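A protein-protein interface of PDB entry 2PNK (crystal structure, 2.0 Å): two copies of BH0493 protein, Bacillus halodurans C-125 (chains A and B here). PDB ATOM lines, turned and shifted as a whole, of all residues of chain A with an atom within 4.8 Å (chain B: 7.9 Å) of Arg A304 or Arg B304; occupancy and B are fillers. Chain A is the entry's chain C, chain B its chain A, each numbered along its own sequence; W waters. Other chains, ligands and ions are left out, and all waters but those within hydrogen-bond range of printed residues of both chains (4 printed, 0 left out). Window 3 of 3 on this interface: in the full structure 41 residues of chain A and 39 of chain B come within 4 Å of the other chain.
Arg B304 touches its own counterpart, Arg A304. His A308 touches Met B329, but with the chains exchanged Met A329 does not touch His B308 (16.6 Å). Glu A337 touches Arg B304, but with the chains exchanged Arg A304 does not touch Glu B337 (5.2 Å). Met A341 touches Arg B304, but with the chains exchanged Arg A304 does not touch Met B341 (8.2 Å). Positions printed for both chains: 302, 303, 304, 305, 306, 307, 308, 329, 337 and 341. Of the 8 pairs that touch across the chains among the printed residues, 2 have their exchanged pair printed and touching as well.
Arg A304 touches Arg B304. Met B329 touches His A308 (CE to CE1, 3.0 Å). CD2 of His A308 touches CD1 of Ile B334, at 3.4 Å. Glu A337 touches Glu B333 (CB to OE2, 3.9 Å). Arg B304 touches Met A341 (NH1 to CE, 3.7 Å).
Water W1 lies within hydrogen-bond range of the side-chain carboxylate of Glu B305 (2.7 Å), the backbone carbonyl oxygen of Glu A305 (2.9 Å) and the backbone NH of His A308 (3.3 Å). Water W2 lies within hydrogen-bond range of OE2 of Glu A337 (2.7 Å), NH1 of Arg B304 (3.3 Å) and O of Arg A304 (3.4 Å). Water W3 lies within hydrogen-bond range of OE2 of Glu B305, O of Arg A304, NH1 of Arg B304 and N of His A308. Water W4 lies within hydrogen-bond range of ND1 of His A308 (2.9 Å), OE1 of Glu B305 (2.9 Å), N of Arg B304 (2.9 Å) and OG of Ser B303 (3.3 Å).
OG of Ser A303 lies close to N of Glu A305 (3.2 Å). The guanidinium group of Arg B304 lies within salt-bridge range of the side-chain carboxylate of Glu B337, 3.0 Å away. The backbone NH of Arg B304 lies close to the side-chain sulfur of Met B329 (3.6 Å). The guanidinium group of Arg A304 lies within salt-bridge range of the side-chain carboxylate of Glu A337, at 2.8 Å. The side-chain hydroxyl (OG) of Ser B303 sits close to the backbone NH (N) of Glu B305. The backbone NH of Arg A304 sits close to the side-chain sulfur of Met A329 (3.7 Å).
The side-chain carboxylate (OE1) of Glu B305 sits close to the backbone carbonyl oxygen (O) of Glu A305 (3.5 Å). A ring nitrogen (NE2) of His A308 lies within hydrogen-bond range of the backbone carbonyl oxygen of Phe B328 (2.9 Å). NH1 of Arg B304 is in salt-bridge range of OE2 of Glu A337.
Arg A304 touches just one residue of chain B: Arg B304 (3.7 Å). Of chain A, only Arg A304 (3.7 Å), Glu A337 (3.2 Å) and Met A341 (3.7 Å) come within 4 Å of Arg B304. No residue of chain B comes within 4 Å of Ser A303. Printed residues of chain A within 4 Å of Glu B333: Glu A337 (3.9 Å). Printed residues of chain B within 4 Å of Glu A337: Arg B304 (3.2 Å) and Glu B333 (3.9 Å). Of the printed residues of chain B, His A308 touches Phe B328, Met B329 and Ile B334. Met B341 touches none of the printed residues of chain A. Asn B306 touches none of the printed residues of chain A. The nearest residue of chain A that does not touch Arg B304 is His A308 (4.02 Å).
Printed residues of chain B that touch a printed residue of chain A: Arg B304, Glu B305, Phe B328, Met B329, Glu B333 and Ile B334. Among the printed residues, 8 pairs touch across the chains. Among the printed residues, Asp or Glu carboxylates within 4 Å of a Lys or Arg side-chain nitrogen of the other chain: Glu A337 with Arg B304 (3.2 Å).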
ATOM      1  N   LEU A 302       2.503  -0.985  34.239  1.00  0.00           N
ATOM      2  CA  LEU A 302       1.851  -1.462  35.447  1.00  0.00           C
ATOM      3  C   LEU A 302       1.103  -2.754  35.279  1.00  0.00           C
ATOM      4  O   LEU A 302       0.938  -3.479  36.245  1.00  0.00           O
ATOM      5  CB  LEU A 302       0.883  -0.418  35.972  1.00  0.00           C
ATOM      6  CG  LEU A 302       0.500  -0.527  37.454  1.00  0.00           C
ATOM      7  CD1 LEU A 302       1.705  -0.677  38.382  1.00  0.00           C
ATOM      8  CD2 LEU A 302      -0.396   0.662  37.819  1.00  0.00           C
ATOM      9  N   SER A 303       0.616  -3.006  34.058  1.00  0.00           N
ATOM     10  CA  SER A 303      -0.168  -4.190  33.739  1.00  0.00           C
ATOM     11  C   SER A 303       0.698  -5.413  33.486  1.00  0.00           C
ATOM     12  O   SER A 303       1.674  -5.357  32.753  1.00  0.00           O
ATOM     13  CB  SER A 303      -1.031  -3.918  32.492  1.00  0.00           C
ATOM     14  OG  SER A 303      -1.826  -5.048  32.169  1.00  0.00           O
ATOM     15  N   ARG A 304       0.336  -6.543  34.082  1.00  0.00           N
ATOM     16  CA  ARG A 304       1.066  -7.774  33.815  1.00  0.00           C
ATOM     17  C   ARG A 304       1.102  -8.048  32.316  1.00  0.00           C
ATOM     18  O   ARG A 304       2.106  -8.534  31.763  1.00  0.00           O
ATOM     19  CB  ARG A 304       0.385  -8.950  34.540  1.00  0.00           C
ATOM     20  CG  ARG A 304       1.179 -10.229  34.499  1.00  0.00           C
ATOM     21  CD  ARG A 304       0.383 -11.392  35.024  1.00  0.00           C
ATOM     22  NE  ARG A 304       1.171 -12.620  34.956  1.00  0.00           N
ATOM     23  CZ  ARG A 304       0.655 -13.848  34.954  1.00  0.00           C
ATOM     24  NH1 ARG A 304      -0.659 -14.040  34.996  1.00  0.00           N
ATOM     25  NH2 ARG A 304       1.462 -14.902  34.883  1.00  0.00           N
ATOM     26  N   GLU A 305       0.005  -7.677  31.662  1.00  0.00           N
ATOM     27  CA  GLU A 305      -0.257  -8.028  30.279  1.00  0.00           C
ATOM     28  C   GLU A 305       0.477  -7.164  29.248  1.00  0.00           C
ATOM     29  O   GLU A 305       0.484  -7.483  28.069  1.00  0.00           O
ATOM     30  CB  GLU A 305      -1.784  -8.000  30.075  1.00  0.00           C
ATOM     31  CG  GLU A 305      -2.451  -9.238  30.673  1.00  0.00           C
ATOM     32  CD  GLU A 305      -2.561  -9.246  32.201  1.00  0.00           C
ATOM     33  OE1 GLU A 305      -2.799  -8.178  32.822  1.00  0.00           O
ATOM     34  OE2 GLU A 305      -2.431 -10.353  32.788  1.00  0.00           O
ATOM     35  N   ASN A 306       1.148  -6.109  29.706  1.00  0.00           N
ATOM     36  CA  ASN A 306       2.052  -5.310  28.854  1.00  0.00           C
ATOM     37  C   ASN A 306       3.501  -5.757  28.897  1.00  0.00           C
ATOM     38  O   ASN A 306       4.315  -5.324  28.061  1.00  0.00           O
ATOM     39  CB  ASN A 306       2.019  -3.836  29.275  1.00  0.00           C
ATOM     40  CG  ASN A 306       0.847  -3.079  28.718  1.00  0.00           C
ATOM     41  OD1 ASN A 306       0.193  -2.386  29.458  1.00  0.00           O
ATOM     42  ND2 ASN A 306       0.570  -3.196  27.390  1.00  0.00           N
ATOM     43  N   GLN A 307       3.855  -6.637  29.829  1.00  0.00           N
ATOM     44  CA  GLN A 307       5.290  -6.816  30.147  1.00  0.00           C
ATOM     45  C   GLN A 307       6.073  -7.470  29.025  1.00  0.00           C
ATOM     46  O   GLN A 307       7.167  -7.007  28.696  1.00  0.00           O
ATOM     47  CB  GLN A 307       5.529  -7.552  31.487  1.00  0.00           C
ATOM     48  CG  GLN A 307       4.937  -6.892  32.731  1.00  0.00           C
ATOM     49  CD  GLN A 307       5.387  -5.470  32.889  1.00  0.00           C
ATOM     50  OE1 GLN A 307       6.514  -5.106  32.497  1.00  0.00           O
ATOM     51  NE2 GLN A 307       4.484  -4.619  33.398  1.00  0.00           N
ATOM     52  N   HIS A 308       5.527  -8.511  28.408  1.00  0.00           N
ATOM     53  CA  HIS A 308       6.273  -9.191  27.335  1.00  0.00           C
ATOM     54  C   HIS A 308       6.447  -8.321  26.097  1.00  0.00           C
ATOM     55  O   HIS A 308       7.564  -8.251  25.490  1.00  0.00           O
ATOM     56  CB  HIS A 308       5.601 -10.524  26.964  1.00  0.00           C
ATOM     57  CG  HIS A 308       6.222 -11.198  25.773  1.00  0.00           C
ATOM     58  ND1 HIS A 308       5.833 -10.935  24.478  1.00  0.00           N
ATOM     59  CD2 HIS A 308       7.197 -12.134  25.688  1.00  0.00           C
ATOM     60  CE1 HIS A 308       6.531 -11.689  23.648  1.00  0.00           C
ATOM     61  NE2 HIS A 308       7.391 -12.399  24.357  1.00  0.00           N
ATOM     62  N   MET A 329       3.298  -4.837  40.045  1.00  0.00           N
ATOM     63  CA  MET A 329       4.238  -5.819  39.479  1.00  0.00           C
ATOM     64  C   MET A 329       5.301  -6.228  40.500  1.00  0.00           C
ATOM     65  O   MET A 329       6.067  -7.172  40.253  1.00  0.00           O
ATOM     66  CB  MET A 329       4.985  -5.261  38.258  1.00  0.00           C
ATOM     67  CG  MET A 329       4.120  -4.774  37.096  1.00  0.00           C
ATOM     68  SD  MET A 329       3.301  -6.216  36.194  1.00  0.00           S
ATOM     69  CE  MET A 329       1.683  -6.347  37.189  1.00  0.00           C
ATOM     70  N   GLU A 337       9.008 -13.902  36.669  1.00  0.00           N
ATOM     71  CA  GLU A 337       8.662 -14.100  35.270  1.00  0.00           C
ATOM     72  C   GLU A 337       9.122 -12.950  34.415  1.00  0.00           C
ATOM     73  O   GLU A 337       9.613 -13.158  33.302  1.00  0.00           O
ATOM     74  CB  GLU A 337       7.144 -14.352  35.080  1.00  0.00           C
ATOM     75  CG  GLU A 337       6.258 -13.137  35.199  1.00  0.00           C
ATOM     76  CD  GLU A 337       4.755 -13.417  34.968  1.00  0.00           C
ATOM     77  OE1 GLU A 337       4.253 -14.524  35.258  1.00  0.00           O
ATOM     78  OE2 GLU A 337       4.071 -12.507  34.477  1.00  0.00           O
ATOM     79  N   MET A 341      11.940 -13.308  31.399  1.00  0.00           N
ATOM     80  CA  MET A 341      11.643 -12.895  30.019  1.00  0.00           C
ATOM     81  C   MET A 341      12.586 -11.827  29.498  1.00  0.00           C
ATOM     82  O   MET A 341      13.052 -11.855  28.343  1.00  0.00           O
ATOM     83  CB  MET A 341      10.218 -12.347  29.929  1.00  0.00           C
ATOM     84  CG  MET A 341       9.178 -13.436  30.066  1.00  0.00           C
ATOM     85  SD  MET A 341       7.343 -12.771  29.698  1.00  0.00           S
ATOM     86  CE  MET A 341       7.139 -11.315  30.803  1.00  0.00           C
ATOM     87  N   VAL B 277       5.069  -7.016  17.799  1.00  0.00           N
ATOM     88  CA  VAL B 277       4.017  -7.923  18.158  1.00  0.00           C
ATOM     89  C   VAL B 277       2.803  -7.189  18.729  1.00  0.00           C
ATOM     90  O   VAL B 277       2.926  -6.139  19.369  1.00  0.00           O
ATOM     91  CB  VAL B 277       4.527  -8.950  19.214  1.00  0.00           C
ATOM     92  CG1 VAL B 277       4.989  -8.263  20.513  1.00  0.00           C
ATOM     93  CG2 VAL B 277       3.471  -9.979  19.520  1.00  0.00           C
ATOM     94  N   GLY B 278       1.632  -7.786  18.520  1.00  0.00           N
ATOM     95  CA  GLY B 278       0.437  -7.362  19.189  1.00  0.00           C
ATOM     96  C   GLY B 278      -0.495  -8.529  19.426  1.00  0.00           C
ATOM     97  O   GLY B 278      -0.488  -9.521  18.679  1.00  0.00           O
ATOM     98  N   LYS B 279      -1.349  -8.372  20.421  1.00  0.00           N
ATOM     99  CA  LYS B 279      -2.391  -9.333  20.689  1.00  0.00           C
ATOM    100  C   LYS B 279      -3.466  -9.275  19.607  1.00  0.00           C
ATOM    101  O   LYS B 279      -3.889  -8.208  19.176  1.00  0.00           O
ATOM    102  CB  LYS B 279      -3.012  -9.096  22.052  1.00  0.00           C
ATOM    103  CG  LYS B 279      -4.003 -10.176  22.461  1.00  0.00           C
ATOM    104  CD  LYS B 279      -4.682  -9.788  23.758  1.00  0.00           C
ATOM    105  CE  LYS B 279      -5.571 -10.942  24.274  1.00  0.00           C
ATOM    106  NZ  LYS B 279      -6.345 -10.541  25.489  1.00  0.00           N
ATOM    107  N   MET B 301       0.650 -18.363  17.408  1.00  0.00           N
ATOM    108  CA  MET B 301       0.415 -16.943  17.682  1.00  0.00           C
ATOM    109  C   MET B 301       1.588 -16.285  18.411  1.00  0.00           C
ATOM    110  O   MET B 301       2.339 -16.968  19.139  1.00  0.00           O
ATOM    111  CB  MET B 301      -0.899 -16.773  18.429  1.00  0.00           C
ATOM    112  CG  MET B 301      -2.094 -17.201  17.531  1.00  0.00           C
ATOM    113  SD  MET B 301      -3.752 -16.824  18.346  1.00  0.00           S
ATOM    114  CE  MET B 301      -3.911 -14.998  17.640  1.00  0.00           C
ATOM    115  N   LEU B 302       1.749 -14.967  18.192  1.00  0.00           N
ATOM    116  CA  LEU B 302       2.995 -14.289  18.511  1.00  0.00           C
ATOM    117  C   LEU B 302       2.983 -13.643  19.906  1.00  0.00           C
ATOM    118  O   LEU B 302       4.038 -13.478  20.508  1.00  0.00           O
ATOM    119  CB  LEU B 302       3.356 -13.238  17.431  1.00  0.00           C
ATOM    120  CG  LEU B 302       4.772 -12.647  17.512  1.00  0.00           C
ATOM    121  CD1 LEU B 302       5.836 -13.785  17.569  1.00  0.00           C
ATOM    122  CD2 LEU B 302       5.086 -11.651  16.376  1.00  0.00           C
ATOM    123  N   SER B 303       1.788 -13.344  20.414  1.00  0.00           N
ATOM    124  CA  SER B 303       1.615 -12.600  21.648  1.00  0.00           C
ATOM    125  C   SER B 303       1.448 -13.576  22.802  1.00  0.00           C
ATOM    126  O   SER B 303       0.740 -14.577  22.682  1.00  0.00           O
ATOM    127  CB  SER B 303       0.370 -11.707  21.537  1.00  0.00           C
ATOM    128  OG  SER B 303       0.040 -11.106  22.767  1.00  0.00           O
ATOM    129  N   ARG B 304       2.105 -13.273  23.928  1.00  0.00           N
ATOM    130  CA  ARG B 304       1.995 -14.088  25.127  1.00  0.00           C
ATOM    131  C   ARG B 304       0.542 -14.176  25.557  1.00  0.00           C
ATOM    132  O   ARG B 304       0.052 -15.201  26.054  1.00  0.00           O
ATOM    133  CB  ARG B 304       2.820 -13.440  26.247  1.00  0.00           C
ATOM    134  CG  ARG B 304       2.980 -14.333  27.426  1.00  0.00           C
ATOM    135  CD  ARG B 304       3.533 -13.569  28.587  1.00  0.00           C
ATOM    136  NE  ARG B 304       3.596 -14.432  29.751  1.00  0.00           N
ATOM    137  CZ  ARG B 304       3.727 -14.008  30.997  1.00  0.00           C
ATOM    138  NH1 ARG B 304       3.760 -12.711  31.276  1.00  0.00           N
ATOM    139  NH2 ARG B 304       3.812 -14.894  31.980  1.00  0.00           N
ATOM    140  N   GLU B 305      -0.149 -13.070  25.350  1.00  0.00           N
ATOM    141  CA  GLU B 305      -1.496 -12.874  25.821  1.00  0.00           C
ATOM    142  C   GLU B 305      -2.587 -13.594  25.004  1.00  0.00           C
ATOM    143  O   GLU B 305      -3.744 -13.689  25.466  1.00  0.00           O
ATOM    144  CB  GLU B 305      -1.767 -11.381  25.959  1.00  0.00           C
ATOM    145  CG  GLU B 305      -1.105 -10.765  27.187  1.00  0.00           C
ATOM    146  CD  GLU B 305       0.425 -10.640  27.074  1.00  0.00           C
ATOM    147  OE1 GLU B 305       0.937 -10.228  25.995  1.00  0.00           O
ATOM    148  OE2 GLU B 305       1.107 -10.986  28.077  1.00  0.00           O
ATOM    149  N   ASN B 306      -2.211 -14.198  23.880  1.00  0.00           N
ATOM    150  CA  ASN B 306      -3.120 -15.065  23.142  1.00  0.00           C
ATOM    151  C   ASN B 306      -2.990 -16.547  23.451  1.00  0.00           C
ATOM    152  O   ASN B 306      -3.748 -17.347  22.927  1.00  0.00           O
ATOM    153  CB  ASN B 306      -2.948 -14.872  21.635  1.00  0.00           C
ATOM    154  CG  ASN B 306      -3.611 -13.593  21.097  1.00  0.00           C
ATOM    155  OD1 ASN B 306      -2.979 -12.869  20.350  1.00  0.00           O
ATOM    156  ND2 ASN B 306      -4.886 -13.345  21.433  1.00  0.00           N
ATOM    157  N   GLN B 307      -2.003 -16.944  24.258  1.00  0.00           N
ATOM    158  CA  GLN B 307      -1.627 -18.339  24.280  1.00  0.00           C
ATOM    159  C   GLN B 307      -2.632 -19.200  24.972  1.00  0.00           C
ATOM    160  O   GLN B 307      -2.956 -20.245  24.470  1.00  0.00           O
ATOM    161  CB  GLN B 307      -0.248 -18.541  24.903  1.00  0.00           C
ATOM    162  CG  GLN B 307       0.854 -17.886  24.115  1.00  0.00           C
ATOM    163  CD  GLN B 307       0.822 -18.239  22.648  1.00  0.00           C
ATOM    164  OE1 GLN B 307       0.454 -19.364  22.266  1.00  0.00           O
ATOM    165  NE2 GLN B 307       1.248 -17.279  21.803  1.00  0.00           N
ATOM    166  N   HIS B 308      -3.161 -18.743  26.097  1.00  0.00           N
ATOM    167  CA  HIS B 308      -4.123 -19.548  26.829  1.00  0.00           C
ATOM    168  C   HIS B 308      -5.399 -19.689  26.041  1.00  0.00           C
ATOM    169  O   HIS B 308      -5.975 -20.755  26.011  1.00  0.00           O
ATOM    170  CB  HIS B 308      -4.377 -19.000  28.243  1.00  0.00           C
ATOM    171  CG  HIS B 308      -5.494 -19.702  28.952  1.00  0.00           C
ATOM    172  ND1 HIS B 308      -6.805 -19.315  28.806  1.00  0.00           N
ATOM    173  CD2 HIS B 308      -5.512 -20.805  29.739  1.00  0.00           C
ATOM    174  CE1 HIS B 308      -7.585 -20.136  29.490  1.00  0.00           C
ATOM    175  NE2 HIS B 308      -6.826 -21.046  30.074  1.00  0.00           N
ATOM    176  N   GLU B 309      -5.862 -18.608  25.403  1.00  0.00           N
ATOM    177  CA  GLU B 309      -7.154 -18.657  24.711  1.00  0.00           C
ATOM    178  C   GLU B 309      -7.079 -19.507  23.411  1.00  0.00           C
ATOM    179  O   GLU B 309      -8.066 -20.137  23.009  1.00  0.00           O
ATOM    180  CB  GLU B 309      -7.760 -17.257  24.518  1.00  0.00           C
ATOM    181  CG  GLU B 309      -6.986 -16.357  23.601  1.00  0.00           C
ATOM    182  CD  GLU B 309      -7.394 -14.896  23.705  1.00  0.00           C
ATOM    183  OE1 GLU B 309      -8.294 -14.536  24.474  1.00  0.00           O
ATOM    184  OE2 GLU B 309      -6.816 -14.090  22.960  1.00  0.00           O
ATOM    185  N   PHE B 328       9.130 -14.502  19.369  1.00  0.00           N
ATOM    186  CA  PHE B 328       9.240 -13.889  20.688  1.00  0.00           C
ATOM    187  C   PHE B 328       8.702 -14.805  21.790  1.00  0.00           C
ATOM    188  O   PHE B 328       8.885 -14.535  22.977  1.00  0.00           O
ATOM    189  CB  PHE B 328       8.564 -12.502  20.730  1.00  0.00           C
ATOM    190  CG  PHE B 328       9.057 -11.550  19.653  1.00  0.00           C
ATOM    191  CD1 PHE B 328      10.406 -11.182  19.584  1.00  0.00           C
ATOM    192  CD2 PHE B 328       8.196 -11.042  18.707  1.00  0.00           C
ATOM    193  CE1 PHE B 328      10.868 -10.347  18.575  1.00  0.00           C
ATOM    194  CE2 PHE B 328       8.646 -10.159  17.688  1.00  0.00           C
ATOM    195  CZ  PHE B 328       9.988  -9.829  17.632  1.00  0.00           C
ATOM    196  N   MET B 329       7.985 -15.860  21.414  1.00  0.00           N
ATOM    197  CA  MET B 329       7.589 -16.893  22.376  1.00  0.00           C
ATOM    198  C   MET B 329       8.713 -17.926  22.591  1.00  0.00           C
ATOM    199  O   MET B 329       8.653 -18.733  23.537  1.00  0.00           O
ATOM    200  CB  MET B 329       6.317 -17.621  21.897  1.00  0.00           C
ATOM    201  CG  MET B 329       5.083 -16.704  21.629  1.00  0.00           C
ATOM    202  SD  MET B 329       4.312 -16.084  23.219  1.00  0.00           S
ATOM    203  CE  MET B 329       5.204 -14.357  23.450  1.00  0.00           C
ATOM    204  N   GLU B 333      11.270 -19.299  29.501  1.00  0.00           N
ATOM    205  CA  GLU B 333      10.200 -18.992  30.441  1.00  0.00           C
ATOM    206  C   GLU B 333       8.830 -19.211  29.800  1.00  0.00           C
ATOM    207  O   GLU B 333       7.910 -19.741  30.438  1.00  0.00           O
ATOM    208  CB  GLU B 333      10.316 -17.538  30.900  1.00  0.00           C
ATOM    209  CG  GLU B 333       9.422 -17.111  32.035  1.00  0.00           C
ATOM    210  CD  GLU B 333       9.520 -17.941  33.321  1.00  0.00           C
ATOM    211  OE1 GLU B 333      10.524 -18.679  33.548  1.00  0.00           O
ATOM    212  OE2 GLU B 333       8.559 -17.819  34.127  1.00  0.00           O
ATOM    213  N   ILE B 334       8.727 -18.827  28.531  1.00  0.00           N
ATOM    214  CA  ILE B 334       7.476 -18.851  27.821  1.00  0.00           C
ATOM    215  C   ILE B 334       7.215 -20.234  27.257  1.00  0.00           C
ATOM    216  O   ILE B 334       6.099 -20.713  27.373  1.00  0.00           O
ATOM    217  CB  ILE B 334       7.423 -17.762  26.735  1.00  0.00           C
ATOM    218  CG1 ILE B 334       7.487 -16.369  27.357  1.00  0.00           C
ATOM    219  CG2 ILE B 334       6.114 -17.858  25.948  1.00  0.00           C
ATOM    220  CD1 ILE B 334       8.004 -15.341  26.402  1.00  0.00           C
ATOM    221  N   GLU B 337       5.766 -22.275  30.221  1.00  0.00           N
ATOM    222  CA  GLU B 337       4.373 -22.027  30.617  1.00  0.00           C
ATOM    223  C   GLU B 337       3.373 -22.484  29.519  1.00  0.00           C
ATOM    224  O   GLU B 337       2.316 -23.055  29.811  1.00  0.00           O
ATOM    225  CB  GLU B 337       4.153 -20.561  31.022  1.00  0.00           C
ATOM    226  CG  GLU B 337       4.136 -19.579  29.841  1.00  0.00           C
ATOM    227  CD  GLU B 337       3.817 -18.160  30.253  1.00  0.00           C
ATOM    228  OE1 GLU B 337       4.041 -17.793  31.427  1.00  0.00           O
ATOM    229  OE2 GLU B 337       3.340 -17.405  29.393  1.00  0.00           O
ATOM    230  N   MET B 338       3.728 -22.258  28.258  1.00  0.00           N
ATOM    231  CA  MET B 338       2.916 -22.685  27.137  1.00  0.00           C
ATOM    232  C   MET B 338       2.762 -24.187  27.079  1.00  0.00           C
ATOM    233  O   MET B 338       1.638 -24.685  26.915  1.00  0.00           O
ATOM    234  CB  MET B 338       3.511 -22.187  25.802  1.00  0.00           C
ATOM    235  CG  MET B 338       3.316 -20.704  25.600  1.00  0.00           C
ATOM    236  SD  MET B 338       4.089 -20.078  23.900  1.00  0.00           S
ATOM    237  CE  MET B 338       3.233 -21.173  22.615  1.00  0.00           C
ATOM    238  N   MET B 341       0.468 -25.380  30.042  1.00  0.00           N
ATOM    239  CA  MET B 341      -0.954 -25.104  29.729  1.00  0.00           C
ATOM    240  C   MET B 341      -1.522 -26.006  28.628  1.00  0.00           C
ATOM    241  O   MET B 341      -2.615 -26.586  28.738  1.00  0.00           O
ATOM    242  CB  MET B 341      -1.143 -23.638  29.326  1.00  0.00           C
ATOM    243  CG  MET B 341      -0.976 -22.695  30.482  1.00  0.00           C
ATOM    244  SD  MET B 341      -1.367 -20.847  30.008  1.00  0.00           S
ATOM    245  CE  MET B 341      -0.379 -20.750  28.530  1.00  0.00           C
HETATM  246  O   HOH W   1       2.797  -8.414  26.585  1.00  0.00           O
HETATM  247  O   HOH W   2       4.742 -10.219  33.149  1.00  0.00           O
HETATM  248  O   HOH W   3       3.200 -10.193  29.650  1.00  0.00           O
HETATM  249  O   HOH W   4       3.043 -10.480  24.038  1.00  0.00           O
